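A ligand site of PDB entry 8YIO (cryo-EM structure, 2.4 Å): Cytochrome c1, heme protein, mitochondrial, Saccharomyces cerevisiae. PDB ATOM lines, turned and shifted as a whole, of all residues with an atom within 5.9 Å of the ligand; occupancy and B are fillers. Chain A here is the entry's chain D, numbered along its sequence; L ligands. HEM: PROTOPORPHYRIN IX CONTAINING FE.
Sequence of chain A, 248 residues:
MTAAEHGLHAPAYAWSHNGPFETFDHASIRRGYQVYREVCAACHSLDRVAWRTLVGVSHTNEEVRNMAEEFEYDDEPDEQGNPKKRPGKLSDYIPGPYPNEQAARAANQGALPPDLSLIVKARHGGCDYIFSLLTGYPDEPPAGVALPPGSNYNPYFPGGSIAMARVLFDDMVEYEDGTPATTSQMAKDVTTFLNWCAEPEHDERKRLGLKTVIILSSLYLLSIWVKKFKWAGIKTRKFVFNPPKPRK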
ATOM      1  N   VAL A  35      -1.023  15.099  -7.255  1.00  0.00           N
ATOM      2  CA  VAL A  35      -1.398  16.341  -7.924  1.00  0.00           C
ATOM      3  C   VAL A  35      -0.170  17.006  -8.551  1.00  0.00           C
ATOM      4  O   VAL A  35      -0.280  17.701  -9.572  1.00  0.00           O
ATOM      5  CB  VAL A  35      -2.133  17.275  -6.932  1.00  0.00           C
ATOM      6  CG1 VAL A  35      -2.785  18.446  -7.655  1.00  0.00           C
ATOM      7  CG2 VAL A  35      -3.175  16.499  -6.168  1.00  0.00           C
ATOM      8  N   VAL A  39      -0.368  17.440 -12.706  1.00  0.00           N
ATOM      9  CA  VAL A  39      -0.745  18.807 -13.050  1.00  0.00           C
ATOM     10  C   VAL A  39       0.470  19.729 -13.071  1.00  0.00           C
ATOM     11  O   VAL A  39       0.765  20.348 -14.094  1.00  0.00           O
ATOM     12  CB  VAL A  39      -1.819  19.354 -12.099  1.00  0.00           C
ATOM     13  CG1 VAL A  39      -2.176  20.782 -12.474  1.00  0.00           C
ATOM     14  CG2 VAL A  39      -3.072  18.486 -12.120  1.00  0.00           C
ATOM     15  N   CYS A  40       1.168  19.838 -11.934  1.00  0.00           N
ATOM     16  CA  CYS A  40       2.154  20.910 -11.752  1.00  0.00           C
ATOM     17  C   CYS A  40       3.408  20.672 -12.573  1.00  0.00           C
ATOM     18  O   CYS A  40       4.012  21.628 -13.069  1.00  0.00           O
ATOM     19  CB  CYS A  40       2.541  21.055 -10.280  1.00  0.00           C
ATOM     20  SG  CYS A  40       1.290  20.797  -9.036  1.00  0.00           S
ATOM     21  N   ALA A  42       4.286  19.708 -15.431  1.00  0.00           N
ATOM     22  CA  ALA A  42       4.420  20.081 -16.831  1.00  0.00           C
ATOM     23  C   ALA A  42       5.197  21.378 -17.005  1.00  0.00           C
ATOM     24  O   ALA A  42       5.765  21.598 -18.080  1.00  0.00           O
ATOM     25  CB  ALA A  42       3.045  20.211 -17.480  1.00  0.00           C
ATOM     26  N   CYS A  43       5.246  22.233 -15.991  1.00  0.00           N
ATOM     27  CA  CYS A  43       5.927  23.509 -16.099  1.00  0.00           C
ATOM     28  C   CYS A  43       6.802  23.870 -14.911  1.00  0.00           C
ATOM     29  O   CYS A  43       7.594  24.814 -15.027  1.00  0.00           O
ATOM     30  CB  CYS A  43       4.913  24.634 -16.343  1.00  0.00           C
ATOM     31  SG  CYS A  43       4.190  24.550 -17.992  1.00  0.00           S
ATOM     32  N   HIS A  44       6.717  23.157 -13.800  1.00  0.00           N
ATOM     33  CA  HIS A  44       7.462  23.493 -12.590  1.00  0.00           C
ATOM     34  C   HIS A  44       8.469  22.405 -12.244  1.00  0.00           C
ATOM     35  O   HIS A  44       8.185  21.214 -12.347  1.00  0.00           O
ATOM     36  CB  HIS A  44       6.515  23.710 -11.417  1.00  0.00           C
ATOM     37  CG  HIS A  44       5.967  25.091 -11.353  1.00  0.00           C
ATOM     38  ND1 HIS A  44       6.715  26.172 -10.941  1.00  0.00           N
ATOM     39  CD2 HIS A  44       4.741  25.575 -11.663  1.00  0.00           C
ATOM     40  CE1 HIS A  44       5.976  27.265 -10.989  1.00  0.00           C
ATOM     41  NE2 HIS A  44       4.781  26.927 -11.435  1.00  0.00           N
ATOM     42  N   ASN A 108       6.167  29.596 -22.240  1.00  0.00           N
ATOM     43  CA  ASN A 108       5.203  30.253 -21.351  1.00  0.00           C
ATOM     44  C   ASN A 108       5.096  31.744 -21.648  1.00  0.00           C
ATOM     45  O   ASN A 108       4.893  32.542 -20.725  1.00  0.00           O
ATOM     46  CB  ASN A 108       5.574  30.031 -19.886  1.00  0.00           C
ATOM     47  CG  ASN A 108       5.399  28.591 -19.451  1.00  0.00           C
ATOM     48  OD1 ASN A 108       4.316  28.184 -19.036  1.00  0.00           O
ATOM     49  ND2 ASN A 108       6.471  27.821 -19.528  1.00  0.00           N
ATOM     50  N   ALA A 111       7.334  34.333 -19.684  1.00  0.00           N
ATOM     51  CA  ALA A 111       7.334  34.251 -18.232  1.00  0.00           C
ATOM     52  C   ALA A 111       8.085  33.013 -17.768  1.00  0.00           C
ATOM     53  O   ALA A 111       8.106  31.981 -18.441  1.00  0.00           O
ATOM     54  CB  ALA A 111       5.909  34.233 -17.690  1.00  0.00           C
ATOM     55  N   LEU A 112       8.707  33.119 -16.592  1.00  0.00           N
ATOM     56  CA  LEU A 112       9.500  32.028 -16.032  1.00  0.00           C
ATOM     57  C   LEU A 112       8.810  31.453 -14.804  1.00  0.00           C
ATOM     58  O   LEU A 112       8.700  32.148 -13.782  1.00  0.00           O
ATOM     59  CB  LEU A 112      10.897  32.527 -15.676  1.00  0.00           C
ATOM     60  CG  LEU A 112      11.845  31.490 -15.068  1.00  0.00           C
ATOM     61  CD1 LEU A 112      12.147  30.393 -16.078  1.00  0.00           C
ATOM     62  CD2 LEU A 112      13.133  32.140 -14.587  1.00  0.00           C
ATOM     63  N   PRO A 113       8.333  30.208 -14.850  1.00  0.00           N
ATOM     64  CA  PRO A 113       7.753  29.593 -13.647  1.00  0.00           C
ATOM     65  C   PRO A 113       8.846  29.216 -12.663  1.00  0.00           C
ATOM     66  O   PRO A 113       9.806  28.532 -13.029  1.00  0.00           O
ATOM     67  CB  PRO A 113       7.034  28.355 -14.199  1.00  0.00           C
ATOM     68  CG  PRO A 113       7.103  28.460 -15.697  1.00  0.00           C
ATOM     69  CD  PRO A 113       8.280  29.312 -16.006  1.00  0.00           C
ATOM     70  N   PRO A 114       8.717  29.621 -11.405  1.00  0.00           N
ATOM     71  CA  PRO A 114       9.803  29.400 -10.446  1.00  0.00           C
ATOM     72  C   PRO A 114       9.842  27.977  -9.902  1.00  0.00           C
ATOM     73  O   PRO A 114       8.859  27.230  -9.954  1.00  0.00           O
ATOM     74  CB  PRO A 114       9.503  30.409  -9.334  1.00  0.00           C
ATOM     75  CG  PRO A 114       8.033  30.597  -9.404  1.00  0.00           C
ATOM     76  CD  PRO A 114       7.644  30.447 -10.839  1.00  0.00           C
ATOM     77  N   LEU A 116       9.695  25.251  -7.068  1.00  0.00           N
ATOM     78  CA  LEU A 116       8.719  25.209  -5.985  1.00  0.00           C
ATOM     79  C   LEU A 116       9.245  24.499  -4.732  1.00  0.00           C
ATOM     80  O   LEU A 116       8.446  24.131  -3.867  1.00  0.00           O
ATOM     81  CB  LEU A 116       7.426  24.532  -6.454  1.00  0.00           C
ATOM     82  CG  LEU A 116       6.589  25.208  -7.548  1.00  0.00           C
ATOM     83  CD1 LEU A 116       5.352  24.386  -7.853  1.00  0.00           C
ATOM     84  CD2 LEU A 116       6.213  26.631  -7.187  1.00  0.00           C
ATOM     85  N   ILE A 119       8.912  27.451  -1.979  1.00  0.00           N
ATOM     86  CA  ILE A 119       7.919  28.482  -2.251  1.00  0.00           C
ATOM     87  C   ILE A 119       7.030  28.813  -1.053  1.00  0.00           C
ATOM     88  O   ILE A 119       6.482  29.910  -0.978  1.00  0.00           O
ATOM     89  CB  ILE A 119       7.083  28.080  -3.493  1.00  0.00           C
ATOM     90  CG1 ILE A 119       6.505  29.314  -4.199  1.00  0.00           C
ATOM     91  CG2 ILE A 119       5.979  27.082  -3.163  1.00  0.00           C
ATOM     92  CD1 ILE A 119       7.532  30.219  -4.782  1.00  0.00           C
ATOM     93  N   ARG A 123       7.366  33.251   0.468  1.00  0.00           N
ATOM     94  CA  ARG A 123       6.271  34.188   0.271  1.00  0.00           C
ATOM     95  C   ARG A 123       5.685  34.560   1.615  1.00  0.00           C
ATOM     96  O   ARG A 123       5.601  33.722   2.525  1.00  0.00           O
ATOM     97  CB  ARG A 123       5.175  33.607  -0.625  1.00  0.00           C
ATOM     98  CG  ARG A 123       5.580  33.357  -2.055  1.00  0.00           C
ATOM     99  CD  ARG A 123       5.895  34.641  -2.784  1.00  0.00           C
ATOM    100  NE  ARG A 123       6.202  34.404  -4.195  1.00  0.00           N
ATOM    101  CZ  ARG A 123       7.408  34.127  -4.654  1.00  0.00           C
ATOM    102  NH1 ARG A 123       7.591  33.917  -5.953  1.00  0.00           N
ATOM    103  NH2 ARG A 123       8.445  34.049  -3.837  1.00  0.00           N
ATOM    104  N   TYR A 129      -1.317  31.685   1.668  1.00  0.00           N
ATOM    105  CA  TYR A 129      -1.210  32.423   0.403  1.00  0.00           C
ATOM    106  C   TYR A 129      -1.253  31.484  -0.795  1.00  0.00           C
ATOM    107  O   TYR A 129      -1.868  31.813  -1.818  1.00  0.00           O
ATOM    108  CB  TYR A 129       0.059  33.269   0.381  1.00  0.00           C
ATOM    109  CG  TYR A 129       0.399  33.788  -0.993  1.00  0.00           C
ATOM    110  CD1 TYR A 129      -0.355  34.807  -1.572  1.00  0.00           C
ATOM    111  CD2 TYR A 129       1.461  33.267  -1.721  1.00  0.00           C
ATOM    112  CE1 TYR A 129      -0.052  35.283  -2.836  1.00  0.00           C
ATOM    113  CE2 TYR A 129       1.762  33.733  -2.981  1.00  0.00           C
ATOM    114  CZ  TYR A 129       1.001  34.735  -3.529  1.00  0.00           C
ATOM    115  OH  TYR A 129       1.297  35.216  -4.781  1.00  0.00           O
ATOM    116  N   ILE A 130      -0.593  30.327  -0.694  1.00  0.00           N
ATOM    117  CA  ILE A 130      -0.566  29.370  -1.808  1.00  0.00           C
ATOM    118  C   ILE A 130      -1.946  28.781  -2.042  1.00  0.00           C
ATOM    119  O   ILE A 130      -2.370  28.591  -3.188  1.00  0.00           O
ATOM    120  CB  ILE A 130       0.486  28.276  -1.533  1.00  0.00           C
ATOM    121  CG1 ILE A 130       1.845  28.892  -1.200  1.00  0.00           C
ATOM    122  CG2 ILE A 130       0.604  27.314  -2.700  1.00  0.00           C
ATOM    123  CD1 ILE A 130       2.495  29.607  -2.355  1.00  0.00           C
ATOM    124  N   LEU A 133      -4.315  31.544  -3.637  1.00  0.00           N
ATOM    125  CA  LEU A 133      -3.992  31.850  -5.022  1.00  0.00           C
ATOM    126  C   LEU A 133      -4.613  30.827  -5.968  1.00  0.00           C
ATOM    127  O   LEU A 133      -5.149  31.205  -7.028  1.00  0.00           O
ATOM    128  CB  LEU A 133      -2.481  31.895  -5.207  1.00  0.00           C
ATOM    129  CG  LEU A 133      -1.943  32.345  -6.568  1.00  0.00           C
ATOM    130  CD1 LEU A 133      -2.066  33.846  -6.727  1.00  0.00           C
ATOM    131  CD2 LEU A 133      -0.494  31.900  -6.728  1.00  0.00           C
ATOM    132  N   LEU A 134      -4.572  29.543  -5.605  1.00  0.00           N
ATOM    133  CA  LEU A 134      -5.048  28.497  -6.503  1.00  0.00           C
ATOM    134  C   LEU A 134      -6.564  28.467  -6.605  1.00  0.00           C
ATOM    135  O   LEU A 134      -7.104  28.173  -7.679  1.00  0.00           O
ATOM    136  CB  LEU A 134      -4.531  27.143  -6.034  1.00  0.00           C
ATOM    137  CG  LEU A 134      -3.025  26.949  -6.111  1.00  0.00           C
ATOM    138  CD1 LEU A 134      -2.593  25.730  -5.324  1.00  0.00           C
ATOM    139  CD2 LEU A 134      -2.595  26.851  -7.565  1.00  0.00           C
ATOM    140  N   PHE A 157      -2.560  38.094  -6.103  1.00  0.00           N
ATOM    141  CA  PHE A 157      -1.265  38.414  -6.684  1.00  0.00           C
ATOM    142  C   PHE A 157      -1.040  39.924  -6.654  1.00  0.00           C
ATOM    143  O   PHE A 157      -1.964  40.686  -6.956  1.00  0.00           O
ATOM    144  CB  PHE A 157      -1.189  37.893  -8.115  1.00  0.00           C
ATOM    145  CG  PHE A 157       0.199  37.839  -8.683  1.00  0.00           C
ATOM    146  CD1 PHE A 157       1.160  36.990  -8.143  1.00  0.00           C
ATOM    147  CD2 PHE A 157       0.550  38.635  -9.762  1.00  0.00           C
ATOM    148  CE1 PHE A 157       2.438  36.946  -8.652  1.00  0.00           C
ATOM    149  CE2 PHE A 157       1.834  38.584 -10.283  1.00  0.00           C
ATOM    150  CZ  PHE A 157       2.768  37.738  -9.723  1.00  0.00           C
ATOM    151  N   PRO A 158       0.142  40.384  -6.263  1.00  0.00           N
ATOM    152  CA  PRO A 158       0.402  41.837  -6.200  1.00  0.00           C
ATOM    153  C   PRO A 158       0.391  42.477  -7.575  1.00  0.00           C
ATOM    154  O   PRO A 158       1.174  42.130  -8.456  1.00  0.00           O
ATOM    155  CB  PRO A 158       1.791  41.916  -5.549  1.00  0.00           C
ATOM    156  CG  PRO A 158       1.975  40.616  -4.856  1.00  0.00           C
ATOM    157  CD  PRO A 158       1.239  39.603  -5.675  1.00  0.00           C
ATOM    158  N   SER A 161      -2.418  41.019 -11.933  1.00  0.00           N
ATOM    159  CA  SER A 161      -2.230  40.418 -13.258  1.00  0.00           C
ATOM    160  C   SER A 161      -1.140  39.365 -13.172  1.00  0.00           C
ATOM    161  O   SER A 161       0.040  39.696 -12.989  1.00  0.00           O
ATOM    162  CB  SER A 161      -1.884  41.497 -14.279  1.00  0.00           C
ATOM    163  OG  SER A 161      -1.617  40.942 -15.549  1.00  0.00           O
ATOM    164  N   ILE A 162      -1.513  38.089 -13.322  1.00  0.00           N
ATOM    165  CA  ILE A 162      -0.587  36.974 -13.185  1.00  0.00           C
ATOM    166  C   ILE A 162      -0.501  36.234 -14.510  1.00  0.00           C
ATOM    167  O   ILE A 162      -1.470  36.209 -15.287  1.00  0.00           O
ATOM    168  CB  ILE A 162      -1.002  36.044 -12.007  1.00  0.00           C
ATOM    169  CG1 ILE A 162       0.146  35.106 -11.600  1.00  0.00           C
ATOM    170  CG2 ILE A 162      -2.287  35.277 -12.305  1.00  0.00           C
ATOM    171  CD1 ILE A 162      -0.144  34.307 -10.360  1.00  0.00           C
ATOM    172  N   ALA A 163       0.670  35.680 -14.811  1.00  0.00           N
ATOM    173  CA  ALA A 163       0.933  35.043 -16.092  1.00  0.00           C
ATOM    174  C   ALA A 163       0.587  33.561 -16.125  1.00  0.00           C
ATOM    175  O   ALA A 163       0.861  32.904 -17.130  1.00  0.00           O
ATOM    176  CB  ALA A 163       2.400  35.226 -16.476  1.00  0.00           C
ATOM    177  N   MET A 164      -0.004  33.010 -15.079  1.00  0.00           N
ATOM    178  CA  MET A 164      -0.497  31.638 -15.091  1.00  0.00           C
ATOM    179  C   MET A 164      -2.016  31.645 -15.037  1.00  0.00           C
ATOM    180  O   MET A 164      -2.623  32.502 -14.390  1.00  0.00           O
ATOM    181  CB  MET A 164       0.087  30.803 -13.945  1.00  0.00           C
ATOM    182  CG  MET A 164      -0.287  31.235 -12.542  1.00  0.00           C
ATOM    183  SD  MET A 164      -0.044  29.936 -11.315  1.00  0.00           S
ATOM    184  CE  MET A 164      -0.801  28.549 -12.158  1.00  0.00           C
ATOM    185  N   VAL A 167      -5.742  26.266 -13.240  1.00  0.00           N
ATOM    186  CA  VAL A 167      -5.381  24.918 -13.660  1.00  0.00           C
ATOM    187  C   VAL A 167      -6.182  23.831 -12.960  1.00  0.00           C
ATOM    188  O   VAL A 167      -6.196  22.692 -13.441  1.00  0.00           O
ATOM    189  CB  VAL A 167      -3.870  24.656 -13.472  1.00  0.00           C
ATOM    190  CG1 VAL A 167      -3.056  25.717 -14.177  1.00  0.00           C
ATOM    191  CG2 VAL A 167      -3.509  24.599 -12.013  1.00  0.00           C
ATOM    192  N   LEU A 168      -6.862  24.120 -11.855  1.00  0.00           N
ATOM    193  CA  LEU A 168      -7.554  23.093 -11.082  1.00  0.00           C
ATOM    194  C   LEU A 168      -9.050  23.122 -11.386  1.00  0.00           C
ATOM    195  O   LEU A 168      -9.688  24.168 -11.235  1.00  0.00           O
ATOM    196  CB  LEU A 168      -7.310  23.281  -9.588  1.00  0.00           C
ATOM    197  CG  LEU A 168      -5.900  22.973  -9.074  1.00  0.00           C
ATOM    198  CD1 LEU A 168      -5.809  23.185  -7.579  1.00  0.00           C
ATOM    199  CD2 LEU A 168      -5.501  21.548  -9.430  1.00  0.00           C
ATOM    200  N   VAL A 190      -1.898  19.588  -2.243  1.00  0.00           N
ATOM    201  CA  VAL A 190      -0.637  19.974  -2.861  1.00  0.00           C
ATOM    202  C   VAL A 190       0.072  21.070  -2.067  1.00  0.00           C
ATOM    203  O   VAL A 190       1.303  21.175  -2.119  1.00  0.00           O
ATOM    204  CB  VAL A 190      -0.858  20.360  -4.332  1.00  0.00           C
ATOM    205  CG1 VAL A 190      -1.576  21.696  -4.473  1.00  0.00           C
ATOM    206  CG2 VAL A 190       0.430  20.312  -5.138  1.00  0.00           C
ATOM    207  N   LEU A 194       3.877  20.640  -0.581  1.00  0.00           N
ATOM    208  CA  LEU A 194       4.892  21.664  -0.787  1.00  0.00           C
ATOM    209  C   LEU A 194       5.463  22.212   0.514  1.00  0.00           C
ATOM    210  O   LEU A 194       6.590  22.706   0.525  1.00  0.00           O
ATOM    211  CB  LEU A 194       4.328  22.800  -1.630  1.00  0.00           C
ATOM    212  CG  LEU A 194       4.174  22.517  -3.130  1.00  0.00           C
ATOM    213  CD1 LEU A 194       3.578  23.701  -3.855  1.00  0.00           C
ATOM    214  CD2 LEU A 194       5.496  22.106  -3.747  1.00  0.00           C
HETATM  215  CHA HEM L   1       3.749  30.862 -10.879  1.00  0.00           C
HETATM  216  CHB HEM L   1       2.239  27.064  -8.284  1.00  0.00           C
HETATM  217  CHC HEM L   1       0.765  24.930 -12.373  1.00  0.00           C
HETATM  218  CHD HEM L   1       2.850  28.415 -14.970  1.00  0.00           C
HETATM  219  C1A HEM L   1       3.433  30.053  -9.817  1.00  0.00           C
HETATM  220  C2A HEM L   1       3.595  30.378  -8.416  1.00  0.00           C
HETATM  221  C3A HEM L   1       3.194  29.336  -7.697  1.00  0.00           C
HETATM  222  C4A HEM L   1       2.740  28.304  -8.608  1.00  0.00           C
HETATM  223  CMA HEM L   1       3.191  29.239  -6.158  1.00  0.00           C
HETATM  224  CAA HEM L   1       4.176  31.687  -7.854  1.00  0.00           C
HETATM  225  CBA HEM L   1       3.134  32.790  -7.717  1.00  0.00           C
HETATM  226  CGA HEM L   1       3.799  33.971  -7.065  1.00  0.00           C
HETATM  227  O1A HEM L   1       4.833  34.450  -7.582  1.00  0.00           O
HETATM  228  O2A HEM L   1       3.282  34.448  -6.026  1.00  0.00           O
HETATM  229  C1B HEM L   1       1.617  26.207  -9.160  1.00  0.00           C
HETATM  230  C2B HEM L   1       0.747  25.107  -8.805  1.00  0.00           C
HETATM  231  C3B HEM L   1       0.344  24.516  -9.945  1.00  0.00           C
HETATM  232  C4B HEM L   1       0.943  25.230 -11.047  1.00  0.00           C
HETATM  233  CMB HEM L   1       0.446  24.760  -7.332  1.00  0.00           C
HETATM  234  CAB HEM L   1      -0.606  23.330 -10.243  1.00  0.00           C
HETATM  235  CBB HEM L   1      -1.534  22.814  -9.430  1.00  0.00           C
HETATM  236  C1C HEM L   1       1.191  25.677 -13.438  1.00  0.00           C
HETATM  237  C2C HEM L   1       0.934  25.392 -14.833  1.00  0.00           C
HETATM  238  C3C HEM L   1       1.506  26.367 -15.564  1.00  0.00           C
HETATM  239  C4C HEM L   1       2.137  27.290 -14.638  1.00  0.00           C
HETATM  240  CMC HEM L   1       0.124  24.143 -15.268  1.00  0.00           C
HETATM  241  CAC HEM L   1       1.589  26.632 -17.096  1.00  0.00           C
HETATM  242  CBC HEM L   1       0.894  26.030 -18.070  1.00  0.00           C
HETATM  243  C1D HEM L   1       3.249  29.395 -14.097  1.00  0.00           C
HETATM  244  C2D HEM L   1       3.813  30.673 -14.459  1.00  0.00           C
HETATM  245  C3D HEM L   1       4.065  31.348 -13.332  1.00  0.00           C
HETATM  246  C4D HEM L   1       3.655  30.525 -12.209  1.00  0.00           C
HETATM  247  CMD HEM L   1       4.085  31.153 -15.895  1.00  0.00           C
HETATM  248  CAD HEM L   1       4.677  32.763 -13.232  1.00  0.00           C
HETATM  249  CBD HEM L   1       3.521  33.752 -13.213  1.00  0.00           C
HETATM  250  CGD HEM L   1       4.001  35.164 -12.996  1.00  0.00           C
HETATM  251  O1D HEM L   1       5.126  35.343 -12.484  1.00  0.00           O
HETATM  252  O2D HEM L   1       3.246  36.107 -13.329  1.00  0.00           O
HETATM  253  NA  HEM L   1       2.900  28.782  -9.889  1.00  0.00           N
HETATM  254  NB  HEM L   1       1.710  26.252 -10.539  1.00  0.00           N
HETATM  255  NC  HEM L   1       1.928  26.830 -13.358  1.00  0.00           N
HETATM  256  ND  HEM L   1       3.154  29.341 -12.713  1.00  0.00           N
HETATM  257 FE   HEM L   1       2.237  27.876 -11.639  1.00  0.00          FE
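The side-chain sulfur (SG) of Cys 43 is in hydrogen-bond range of the side-chain amide oxygen (OD1) of Asn 108 (3.8 Å).
The backbone carbonyl oxygen of Val 35 lies within hydrogen-bond range of the backbone NH of Cys 40 (3.5 Å).
A ring nitrogen (ND1) of His 44 sits at hydrogen-bond distance from the backbone carbonyl oxygen (O) of Pro 114 (2.6 Å).
NE2 of His 44 lies close to NA of the ligand (3.1 Å).
SD of Met 164 sits close to NA of the ligand (3.5 Å).
Val 39 touches the ligand.
Cys 40 touches the ligand.
Cys 43 touches the ligand (SG to CAC, 3.5 Å).
Asn 108 touches the ligand.
Pro 113 touches the ligand (CB to C1D, 3.9 Å).
Pro 114 touches the ligand.
Ile 119 touches the ligand.
Ile 130 touches the ligand (CD1 to CMA, 3.9 Å).
Leu 133 touches the ligand (CD2 to CBA, 3.9 Å).
Leu 134 touches the ligand.
Phe 157 touches the ligand (CE1 to O1A, 3.6 Å).
Ile 162 touches the ligand (CG1 to O2D, 3.7 Å).
Val 167 touches the ligand.
Of the 28 residues printed, 18 come within 4 Å of the ligand.
Along chain A the residues within 4 Å of the ligand span positions 39 to 167.
The nearest printed residue that does not touch the ligand is Ala 111 (4.004 Å).
The side-chain hydroxyl (OH) of Tyr 129 lies within hydrogen-bond range of an oxygen (O2A) of the ligand, 2.5 Å away.
NH1 of Arg 123 lies within salt-bridge range of O1A of the ligand (3.2 Å).
N of Ala 163 is in hydrogen-bond range of O2D of the ligand (3.0 Å).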
